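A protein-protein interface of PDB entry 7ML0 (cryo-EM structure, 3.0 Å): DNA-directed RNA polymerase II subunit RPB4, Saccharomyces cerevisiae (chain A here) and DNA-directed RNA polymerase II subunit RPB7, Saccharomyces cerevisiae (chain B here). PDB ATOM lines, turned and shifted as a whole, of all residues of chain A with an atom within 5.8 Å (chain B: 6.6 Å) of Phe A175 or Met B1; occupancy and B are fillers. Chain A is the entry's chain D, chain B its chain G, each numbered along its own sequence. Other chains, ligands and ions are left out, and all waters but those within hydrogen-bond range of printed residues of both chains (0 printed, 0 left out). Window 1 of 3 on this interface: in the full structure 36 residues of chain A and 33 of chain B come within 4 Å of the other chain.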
ATOM      1  N   ALA A  24     -17.341  -3.403  10.245  1.00  0.00           N
ATOM      2  CA  ALA A  24     -16.720  -3.688   8.959  1.00  0.00           C
ATOM      3  C   ALA A  24     -15.896  -4.957   9.010  1.00  0.00           C
ATOM      4  O   ALA A  24     -16.252  -5.931   9.675  1.00  0.00           O
ATOM      5  CB  ALA A  24     -15.852  -2.529   8.526  1.00  0.00           C
ATOM      6  N   ALA A  25     -14.776  -4.924   8.287  1.00  0.00           N
ATOM      7  CA  ALA A  25     -13.842  -6.042   8.313  1.00  0.00           C
ATOM      8  C   ALA A  25     -13.351  -6.313   9.721  1.00  0.00           C
ATOM      9  O   ALA A  25     -13.247  -7.470  10.132  1.00  0.00           O
ATOM     10  CB  ALA A  25     -12.653  -5.761   7.397  1.00  0.00           C
ATOM     11  N   LEU A  27     -14.408  -6.691  12.361  1.00  0.00           N
ATOM     12  CA  LEU A  27     -15.442  -7.200  13.240  1.00  0.00           C
ATOM     13  C   LEU A  27     -16.123  -6.042  13.954  1.00  0.00           C
ATOM     14  O   LEU A  27     -16.061  -5.886  15.174  1.00  0.00           O
ATOM     15  CB  LEU A  27     -14.886  -8.222  14.227  1.00  0.00           C
ATOM     16  CG  LEU A  27     -14.853  -9.613  13.608  1.00  0.00           C
ATOM     17  CD1 LEU A  27     -14.322 -10.604  14.605  1.00  0.00           C
ATOM     18  CD2 LEU A  27     -16.240 -10.004  13.155  1.00  0.00           C
ATOM     19  N   LEU A  29     -19.792  -5.179  13.317  1.00  0.00           N
ATOM     20  CA  LEU A  29     -21.113  -5.337  12.748  1.00  0.00           C
ATOM     21  C   LEU A  29     -22.054  -4.342  13.412  1.00  0.00           C
ATOM     22  O   LEU A  29     -21.685  -3.627  14.346  1.00  0.00           O
ATOM     23  CB  LEU A  29     -21.593  -6.772  12.917  1.00  0.00           C
ATOM     24  CG  LEU A  29     -20.525  -7.780  12.525  1.00  0.00           C
ATOM     25  CD1 LEU A  29     -20.995  -9.172  12.807  1.00  0.00           C
ATOM     26  CD2 LEU A  29     -20.224  -7.621  11.072  1.00  0.00           C
ATOM     27  N   ALA A  49     -24.414 -17.053  13.760  1.00  0.00           N
ATOM     28  CA  ALA A  49     -23.912 -16.868  12.408  1.00  0.00           C
ATOM     29  C   ALA A  49     -23.712 -18.240  11.794  1.00  0.00           C
ATOM     30  O   ALA A  49     -23.358 -19.191  12.494  1.00  0.00           O
ATOM     31  CB  ALA A  49     -22.611 -16.082  12.391  1.00  0.00           C
ATOM     32  N   LEU A  50     -23.944 -18.351  10.495  1.00  0.00           N
ATOM     33  CA  LEU A  50     -24.107 -19.648   9.863  1.00  0.00           C
ATOM     34  C   LEU A  50     -23.039 -19.903   8.814  1.00  0.00           C
ATOM     35  O   LEU A  50     -22.695 -19.010   8.036  1.00  0.00           O
ATOM     36  CB  LEU A  50     -25.480 -19.748   9.225  1.00  0.00           C
ATOM     37  CG  LEU A  50     -26.590 -19.500  10.231  1.00  0.00           C
ATOM     38  CD1 LEU A  50     -27.922 -19.854   9.633  1.00  0.00           C
ATOM     39  CD2 LEU A  50     -26.354 -20.292  11.500  1.00  0.00           C
ATOM     40  N   HIS A 173     -14.556 -15.293  17.245  1.00  0.00           N
ATOM     41  CA  HIS A 173     -15.805 -14.558  17.097  1.00  0.00           C
ATOM     42  C   HIS A 173     -16.668 -15.203  16.013  1.00  0.00           C
ATOM     43  O   HIS A 173     -16.149 -15.618  14.974  1.00  0.00           O
ATOM     44  CB  HIS A 173     -15.474 -13.104  16.755  1.00  0.00           C
ATOM     45  CG  HIS A 173     -16.645 -12.261  16.369  1.00  0.00           C
ATOM     46  ND1 HIS A 173     -17.451 -12.543  15.290  1.00  0.00           N
ATOM     47  CD2 HIS A 173     -17.099 -11.093  16.882  1.00  0.00           C
ATOM     48  CE1 HIS A 173     -18.382 -11.613  15.184  1.00  0.00           C
ATOM     49  NE2 HIS A 173     -18.185 -10.716  16.132  1.00  0.00           N
ATOM     50  N   PRO A 174     -17.984 -15.289  16.214  1.00  0.00           N
ATOM     51  CA  PRO A 174     -18.807 -16.144  15.339  1.00  0.00           C
ATOM     52  C   PRO A 174     -18.765 -15.763  13.878  1.00  0.00           C
ATOM     53  O   PRO A 174     -18.835 -16.646  13.017  1.00  0.00           O
ATOM     54  CB  PRO A 174     -20.214 -15.977  15.916  1.00  0.00           C
ATOM     55  CG  PRO A 174     -20.003 -15.546  17.297  1.00  0.00           C
ATOM     56  CD  PRO A 174     -18.772 -14.709  17.308  1.00  0.00           C
ATOM     57  N   PHE A 175     -18.663 -14.474  13.566  1.00  0.00           N
ATOM     58  CA  PHE A 175     -18.538 -14.087  12.171  1.00  0.00           C
ATOM     59  C   PHE A 175     -17.299 -14.702  11.551  1.00  0.00           C
ATOM     60  O   PHE A 175     -17.271 -14.972  10.348  1.00  0.00           O
ATOM     61  CB  PHE A 175     -18.494 -12.567  12.036  1.00  0.00           C
ATOM     62  CG  PHE A 175     -18.576 -12.078  10.616  1.00  0.00           C
ATOM     63  CD1 PHE A 175     -19.482 -12.626   9.729  1.00  0.00           C
ATOM     64  CD2 PHE A 175     -17.768 -11.052  10.175  1.00  0.00           C
ATOM     65  CE1 PHE A 175     -19.561 -12.165   8.430  1.00  0.00           C
ATOM     66  CE2 PHE A 175     -17.855 -10.592   8.882  1.00  0.00           C
ATOM     67  CZ  PHE A 175     -18.746 -11.149   8.007  1.00  0.00           C
ATOM     68  N   GLU A 176     -16.265 -14.927  12.352  1.00  0.00           N
ATOM     69  CA  GLU A 176     -15.081 -15.600  11.847  1.00  0.00           C
ATOM     70  C   GLU A 176     -15.349 -17.082  11.663  1.00  0.00           C
ATOM     71  O   GLU A 176     -15.283 -17.604  10.548  1.00  0.00           O
ATOM     72  CB  GLU A 176     -13.926 -15.373  12.810  1.00  0.00           C
ATOM     73  CG  GLU A 176     -14.029 -14.045  13.522  1.00  0.00           C
ATOM     74  CD  GLU A 176     -13.035 -13.913  14.634  1.00  0.00           C
ATOM     75  OE1 GLU A 176     -12.170 -13.023  14.562  1.00  0.00           O
ATOM     76  OE2 GLU A 176     -13.107 -14.710  15.581  1.00  0.00           O
ATOM     77  N   VAL A 177     -15.678 -17.768  12.755  1.00  0.00           N
ATOM     78  CA  VAL A 177     -15.789 -19.220  12.718  1.00  0.00           C
ATOM     79  C   VAL A 177     -16.842 -19.647  11.712  1.00  0.00           C
ATOM     80  O   VAL A 177     -16.699 -20.676  11.046  1.00  0.00           O
ATOM     81  CB  VAL A 177     -16.069 -19.774  14.126  1.00  0.00           C
ATOM     82  CG1 VAL A 177     -15.985 -18.675  15.154  1.00  0.00           C
ATOM     83  CG2 VAL A 177     -17.411 -20.468  14.189  1.00  0.00           C
ATOM     84  N   ALA A 178     -17.917 -18.877  11.580  1.00  0.00           N
ATOM     85  CA  ALA A 178     -18.837 -19.145  10.484  1.00  0.00           C
ATOM     86  C   ALA A 178     -18.193 -18.860   9.143  1.00  0.00           C
ATOM     87  O   ALA A 178     -18.424 -19.593   8.176  1.00  0.00           O
ATOM     88  CB  ALA A 178     -20.109 -18.320  10.635  1.00  0.00           C
ATOM     89  N   GLN A 179     -17.405 -17.792   9.054  1.00  0.00           N
ATOM     90  CA  GLN A 179     -16.768 -17.489   7.784  1.00  0.00           C
ATOM     91  C   GLN A 179     -15.797 -18.590   7.393  1.00  0.00           C
ATOM     92  O   GLN A 179     -15.756 -19.002   6.229  1.00  0.00           O
ATOM     93  CB  GLN A 179     -16.064 -16.137   7.845  1.00  0.00           C
ATOM     94  CG  GLN A 179     -16.843 -14.994   7.206  1.00  0.00           C
ATOM     95  CD  GLN A 179     -16.974 -15.118   5.691  1.00  0.00           C
ATOM     96  OE1 GLN A 179     -17.574 -16.065   5.180  1.00  0.00           O
ATOM     97  NE2 GLN A 179     -16.408 -14.160   4.968  1.00  0.00           N
ATOM     98  N   LEU A 180     -15.024 -19.096   8.350  1.00  0.00           N
ATOM     99  CA  LEU A 180     -14.065 -20.144   8.029  1.00  0.00           C
ATOM    100  C   LEU A 180     -14.765 -21.390   7.523  1.00  0.00           C
ATOM    101  O   LEU A 180     -14.338 -21.995   6.534  1.00  0.00           O
ATOM    102  CB  LEU A 180     -13.218 -20.466   9.253  1.00  0.00           C
ATOM    103  CG  LEU A 180     -12.296 -19.308   9.614  1.00  0.00           C
ATOM    104  CD1 LEU A 180     -11.646 -19.522  10.978  1.00  0.00           C
ATOM    105  CD2 LEU A 180     -11.267 -19.145   8.513  1.00  0.00           C
ATOM    106  N   SER A 182     -17.861 -21.409   6.192  1.00  0.00           N
ATOM    107  CA  SER A 182     -18.490 -21.048   4.934  1.00  0.00           C
ATOM    108  C   SER A 182     -17.501 -21.058   3.783  1.00  0.00           C
ATOM    109  O   SER A 182     -17.891 -21.331   2.644  1.00  0.00           O
ATOM    110  CB  SER A 182     -19.125 -19.654   5.038  1.00  0.00           C
ATOM    111  OG  SER A 182     -20.093 -19.574   6.062  1.00  0.00           O
ATOM    112  N   ILE A 195      -9.665 -13.136   5.259  1.00  0.00           N
ATOM    113  CA  ILE A 195     -10.462 -12.683   6.389  1.00  0.00           C
ATOM    114  C   ILE A 195      -9.537 -11.941   7.336  1.00  0.00           C
ATOM    115  O   ILE A 195      -9.270 -12.416   8.444  1.00  0.00           O
ATOM    116  CB  ILE A 195     -11.160 -13.857   7.072  1.00  0.00           C
ATOM    117  CG1 ILE A 195     -11.643 -14.843   6.013  1.00  0.00           C
ATOM    118  CG2 ILE A 195     -12.323 -13.356   7.883  1.00  0.00           C
ATOM    119  CD1 ILE A 195     -12.398 -16.025   6.575  1.00  0.00           C
ATOM    120  N   MET B   1     -23.826 -12.012   4.415  1.00  0.00           N
ATOM    121  CA  MET B   1     -23.632 -12.961   5.495  1.00  0.00           C
ATOM    122  C   MET B   1     -24.960 -13.406   6.039  1.00  0.00           C
ATOM    123  O   MET B   1     -25.905 -12.628   6.063  1.00  0.00           O
ATOM    124  CB  MET B   1     -22.793 -12.341   6.603  1.00  0.00           C
ATOM    125  CG  MET B   1     -22.719 -13.168   7.864  1.00  0.00           C
ATOM    126  SD  MET B   1     -22.359 -14.896   7.548  1.00  0.00           S
ATOM    127  CE  MET B   1     -21.568 -15.330   9.087  1.00  0.00           C
ATOM    128  N   PHE B   2     -25.032 -14.655   6.486  1.00  0.00           N
ATOM    129  CA  PHE B   2     -26.259 -15.211   7.028  1.00  0.00           C
ATOM    130  C   PHE B   2     -26.236 -15.187   8.544  1.00  0.00           C
ATOM    131  O   PHE B   2     -25.182 -15.316   9.168  1.00  0.00           O
ATOM    132  CB  PHE B   2     -26.476 -16.639   6.548  1.00  0.00           C
ATOM    133  CG  PHE B   2     -26.973 -16.725   5.148  1.00  0.00           C
ATOM    134  CD1 PHE B   2     -26.648 -15.759   4.222  1.00  0.00           C
ATOM    135  CD2 PHE B   2     -27.794 -17.760   4.763  1.00  0.00           C
ATOM    136  CE1 PHE B   2     -27.114 -15.841   2.931  1.00  0.00           C
ATOM    137  CE2 PHE B   2     -28.269 -17.842   3.476  1.00  0.00           C
ATOM    138  CZ  PHE B   2     -27.928 -16.884   2.556  1.00  0.00           C
ATOM    139  N   PHE B   3     -27.416 -14.988   9.126  1.00  0.00           N
ATOM    140  CA  PHE B   3     -27.620 -15.103  10.560  1.00  0.00           C
ATOM    141  C   PHE B   3     -28.996 -15.681  10.808  1.00  0.00           C
ATOM    142  O   PHE B   3     -29.827 -15.780   9.909  1.00  0.00           O
ATOM    143  CB  PHE B   3     -27.561 -13.766  11.283  1.00  0.00           C
ATOM    144  CG  PHE B   3     -26.359 -12.968  10.990  1.00  0.00           C
ATOM    145  CD1 PHE B   3     -26.232 -12.296   9.790  1.00  0.00           C
ATOM    146  CD2 PHE B   3     -25.372 -12.841  11.932  1.00  0.00           C
ATOM    147  CE1 PHE B   3     -25.131 -11.547   9.527  1.00  0.00           C
ATOM    148  CE2 PHE B   3     -24.268 -12.087  11.680  1.00  0.00           C
ATOM    149  CZ  PHE B   3     -24.142 -11.438  10.475  1.00  0.00           C
ATOM    150  N   VAL B  78     -31.454 -14.219   7.906  1.00  0.00           N
ATOM    151  CA  VAL B  78     -31.262 -13.022   7.110  1.00  0.00           C
ATOM    152  C   VAL B  78     -29.886 -13.019   6.491  1.00  0.00           C
ATOM    153  O   VAL B  78     -28.883 -13.262   7.169  1.00  0.00           O
ATOM    154  CB  VAL B  78     -31.437 -11.763   7.951  1.00  0.00           C
ATOM    155  CG1 VAL B  78     -32.878 -11.396   8.017  1.00  0.00           C
ATOM    156  CG2 VAL B  78     -30.901 -12.031   9.314  1.00  0.00           C
ATOM    157  N   PHE B  79     -29.840 -12.706   5.207  1.00  0.00           N
ATOM    158  CA  PHE B  79     -28.591 -12.459   4.518  1.00  0.00           C
ATOM    159  C   PHE B  79     -28.243 -10.997   4.715  1.00  0.00           C
ATOM    160  O   PHE B  79     -28.972 -10.113   4.265  1.00  0.00           O
ATOM    161  CB  PHE B  79     -28.705 -12.795   3.039  1.00  0.00           C
ATOM    162  CG  PHE B  79     -27.558 -12.300   2.242  1.00  0.00           C
ATOM    163  CD1 PHE B  79     -26.284 -12.778   2.479  1.00  0.00           C
ATOM    164  CD2 PHE B  79     -27.742 -11.338   1.275  1.00  0.00           C
ATOM    165  CE1 PHE B  79     -25.231 -12.323   1.760  1.00  0.00           C
ATOM    166  CE2 PHE B  79     -26.689 -10.875   0.549  1.00  0.00           C
ATOM    167  CZ  PHE B  79     -25.428 -11.366   0.791  1.00  0.00           C
ATOM    168  N   LYS B  80     -27.139 -10.745   5.391  1.00  0.00           N
ATOM    169  CA  LYS B  80     -26.752  -9.383   5.735  1.00  0.00           C
ATOM    170  C   LYS B  80     -25.343  -9.077   5.268  1.00  0.00           C
ATOM    171  O   LYS B  80     -24.370  -9.583   5.858  1.00  0.00           O
ATOM    172  CB  LYS B  80     -26.857  -9.174   7.237  1.00  0.00           C
ATOM    173  CG  LYS B  80     -26.199  -7.899   7.688  1.00  0.00           C
ATOM    174  CD  LYS B  80     -26.759  -6.695   6.974  1.00  0.00           C
ATOM    175  CE  LYS B  80     -27.279  -5.687   7.954  1.00  0.00           C
ATOM    176  NZ  LYS B  80     -28.478  -6.225   8.623  1.00  0.00           N
ATOM    177  N   PRO B  81     -25.173  -8.248   4.259  1.00  0.00           N
ATOM    178  CA  PRO B  81     -23.832  -7.871   3.828  1.00  0.00           C
ATOM    179  C   PRO B  81     -23.132  -7.049   4.890  1.00  0.00           C
ATOM    180  O   PRO B  81     -23.722  -6.605   5.871  1.00  0.00           O
ATOM    181  CB  PRO B  81     -24.087  -7.040   2.573  1.00  0.00           C
ATOM    182  CG  PRO B  81     -25.478  -7.376   2.171  1.00  0.00           C
ATOM    183  CD  PRO B  81     -26.208  -7.639   3.425  1.00  0.00           C
ATOM    184  N   PHE B  82     -21.840  -6.848   4.670  1.00  0.00           N
ATOM    185  CA  PHE B  82     -21.043  -5.929   5.467  1.00  0.00           C
ATOM    186  C   PHE B  82     -19.960  -5.358   4.570  1.00  0.00           C
ATOM    187  O   PHE B  82     -20.062  -5.402   3.345  1.00  0.00           O
ATOM    188  CB  PHE B  82     -20.465  -6.627   6.698  1.00  0.00           C
ATOM    189  CG  PHE B  82     -21.486  -6.952   7.722  1.00  0.00           C
ATOM    190  CD1 PHE B  82     -21.956  -5.979   8.566  1.00  0.00           C
ATOM    191  CD2 PHE B  82     -21.994  -8.221   7.825  1.00  0.00           C
ATOM    192  CE1 PHE B  82     -22.901  -6.272   9.504  1.00  0.00           C
ATOM    193  CE2 PHE B  82     -22.940  -8.518   8.758  1.00  0.00           C
ATOM    194  CZ  PHE B  82     -23.390  -7.547   9.602  1.00  0.00           C
ATOM    195  N   LYS B  83     -18.925  -4.795   5.171  1.00  0.00           N
ATOM    196  CA  LYS B  83     -17.769  -4.365   4.406  1.00  0.00           C
ATOM    197  C   LYS B  83     -16.518  -5.026   4.954  1.00  0.00           C
ATOM    198  O   LYS B  83     -16.209  -4.893   6.140  1.00  0.00           O
ATOM    199  CB  LYS B  83     -17.613  -2.853   4.425  1.00  0.00           C
ATOM    200  CG  LYS B  83     -16.685  -2.375   3.347  1.00  0.00           C
ATOM    201  CD  LYS B  83     -16.751  -0.874   3.159  1.00  0.00           C
ATOM    202  CE  LYS B  83     -15.617  -0.179   3.888  1.00  0.00           C
ATOM    203  NZ  LYS B  83     -15.567   1.273   3.579  1.00  0.00           N
ATOM    204  N   GLY B  84     -15.807  -5.738   4.093  1.00  0.00           N
ATOM    205  CA  GLY B  84     -14.512  -6.267   4.434  1.00  0.00           C
ATOM    206  C   GLY B  84     -14.421  -7.742   4.756  1.00  0.00           C
ATOM    207  O   GLY B  84     -13.465  -8.145   5.424  1.00  0.00           O
ATOM    208  N   GLU B  85     -15.359  -8.564   4.295  1.00  0.00           N
ATOM    209  CA  GLU B  85     -15.207 -10.007   4.418  1.00  0.00           C
ATOM    210  C   GLU B  85     -15.596 -10.691   3.116  1.00  0.00           C
ATOM    211  O   GLU B  85     -16.567 -10.303   2.461  1.00  0.00           O
ATOM    212  CB  GLU B  85     -16.027 -10.561   5.574  1.00  0.00           C
ATOM    213  CG  GLU B  85     -15.195 -10.843   6.830  1.00  0.00           C
ATOM    214  CD  GLU B  85     -14.876  -9.592   7.635  1.00  0.00           C
ATOM    215  OE1 GLU B  85     -15.650  -8.615   7.560  1.00  0.00           O
ATOM    216  OE2 GLU B  85     -13.847  -9.588   8.341  1.00  0.00           O
ATOM    217  N   VAL B  86     -14.832 -11.725   2.764  1.00  0.00           N
ATOM    218  CA  VAL B  86     -14.944 -12.371   1.462  1.00  0.00           C
ATOM    219  C   VAL B  86     -16.268 -13.106   1.345  1.00  0.00           C
ATOM    220  O   VAL B  86     -16.712 -13.780   2.281  1.00  0.00           O
ATOM    221  CB  VAL B  86     -13.769 -13.330   1.234  1.00  0.00           C
ATOM    222  CG1 VAL B  86     -12.756 -12.697   0.311  1.00  0.00           C
ATOM    223  CG2 VAL B  86     -13.124 -13.709   2.554  1.00  0.00           C
ATOM    224  N   VAL B  87     -16.897 -12.989   0.185  1.00  0.00           N
ATOM    225  CA  VAL B  87     -18.166 -13.639  -0.107  1.00  0.00           C
ATOM    226  C   VAL B  87     -18.085 -14.232  -1.505  1.00  0.00           C
ATOM    227  O   VAL B  87     -17.466 -13.648  -2.400  1.00  0.00           O
ATOM    228  CB  VAL B  87     -19.339 -12.646   0.004  1.00  0.00           C
ATOM    229  CG1 VAL B  87     -20.649 -13.342  -0.226  1.00  0.00           C
ATOM    230  CG2 VAL B  87     -19.342 -11.986   1.363  1.00  0.00           C
ATOM    231  N   ILE B 147     -16.533  -7.773   0.180  1.00  0.00           N
ATOM    232  CA  ILE B 147     -17.469  -6.667   0.041  1.00  0.00           C
ATOM    233  C   ILE B 147     -16.804  -5.406   0.562  1.00  0.00           C
ATOM    234  O   ILE B 147     -16.428  -5.323   1.735  1.00  0.00           O
ATOM    235  CB  ILE B 147     -18.777  -6.949   0.784  1.00  0.00           C
ATOM    236  CG1 ILE B 147     -19.152  -8.415   0.590  1.00  0.00           C
ATOM    237  CG2 ILE B 147     -19.863  -6.044   0.259  1.00  0.00           C
ATOM    238  CD1 ILE B 147     -20.580  -8.655   0.225  1.00  0.00           C
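The side-chain amide nitrogen (NE2) of Gln A179 lies within hydrogen-bond range of the backbone carbonyl oxygen (O) of Val B86. The backbone NH (N) of Ala A25 sits at hydrogen-bond distance from the backbone carbonyl oxygen (O) of Lys B83, 2.6 Å away. O of Ala A24 lies close to OE1 of Glu B85 (3.5 Å). The backbone carbonyl oxygen of Ala A25 sits close to the side-chain carboxylate of Glu B85 (2.8 Å).
The backbone NH (N) of Ile B147 sits at hydrogen-bond distance from the backbone carbonyl oxygen (O) of Glu B85, at 3.4 Å. The side-chain hydroxyl (OG) of Ser A182 lies within hydrogen-bond range of the backbone carbonyl oxygen (O) of Ala A178 (2.7 Å). OG of Ser A182 sits at hydrogen-bond distance from O of Leu A50 (3.3 Å). The backbone NH of Gly B84 sits at hydrogen-bond distance from the backbone carbonyl oxygen of Ile B147, 2.5 Å away. The backbone NH (N) of Phe A175 sits at hydrogen-bond distance from a ring nitrogen (ND1) of His A173 (2.9 Å). N of Met B1 is in hydrogen-bond range of O of Lys B80 (2.9 Å).
Ala A24 touches Lys B83 (C to O, 2.9 Å). Gly B84 touches Ala A25 (O to CB, 3.2 Å). CD2 of Leu A29 touches CE1 of Phe B82 (3.4 Å). O of Leu A50 touches CE of Met B1, 3.99 Å away. Phe B2 touches Leu A50 (O to N, 3.5 Å). Phe A175 touches Glu B85. Ala A178 touches Met B1. NE2 of Gln A179 touches CB of Glu B85, 3.7 Å away. CG of Glu B85 touches CG2 of Ile A195, at 3.96 Å. Ile A195 touches Val B86.
Phe A175 touches just these residues of chain B: Met B1 and Glu B85. Printed residues of chain A within 4 Å of Met B1: Ala A49 (3.5 Å), Leu A50 (3.99 Å), Phe A175 (3.4 Å) and Ala A178 (3.7 Å). Of the printed residues of chain A, Phe B82 touches Leu A29. Printed residues of chain B within 4 Å of Gln A179: Glu B85 (3.7 Å) and Val B86 (2.7 Å). Of the printed residues of chain A, Val B86 touches Gln A179 (2.7 Å) and Ile A195 (3.9 Å). Of the printed residues of chain B, Ile A195 touches Glu B85 and Val B86. Of the printed residues of chain A, Lys B83 touches Ala A24 and Ala A25. Glu A176 touches none of the printed residues of chain B. Pro A174 touches none of the printed residues of chain B. The nearest printed residue of chain B that does not touch Ala A24 is Gly B84 (5.0 Å).
Hydrophobic or aromatic side chains of chain B within 4 Å of the printed part of chain A: Met B1, Phe B82 and Val B86. Printed residues of chain A that touch a printed residue of chain B: Ala A24, Ala A25, Leu A29, Ala A49, Leu A50, Phe A175, Ala A178, Gln A179 and Ile A195. Hydrophobic or aromatic side chains of chain A that line the printed part of chain B: Ala A24, Ala A25, Leu A29, Ala A49, Phe A175, Ala A178 and Ile A195. Among the printed residues, 17 pairs touch across the chains. Among the printed residues, no Asp or Glu carboxylate lies within 4 Å of a Lys or Arg side-chain nitrogen of the other chain.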
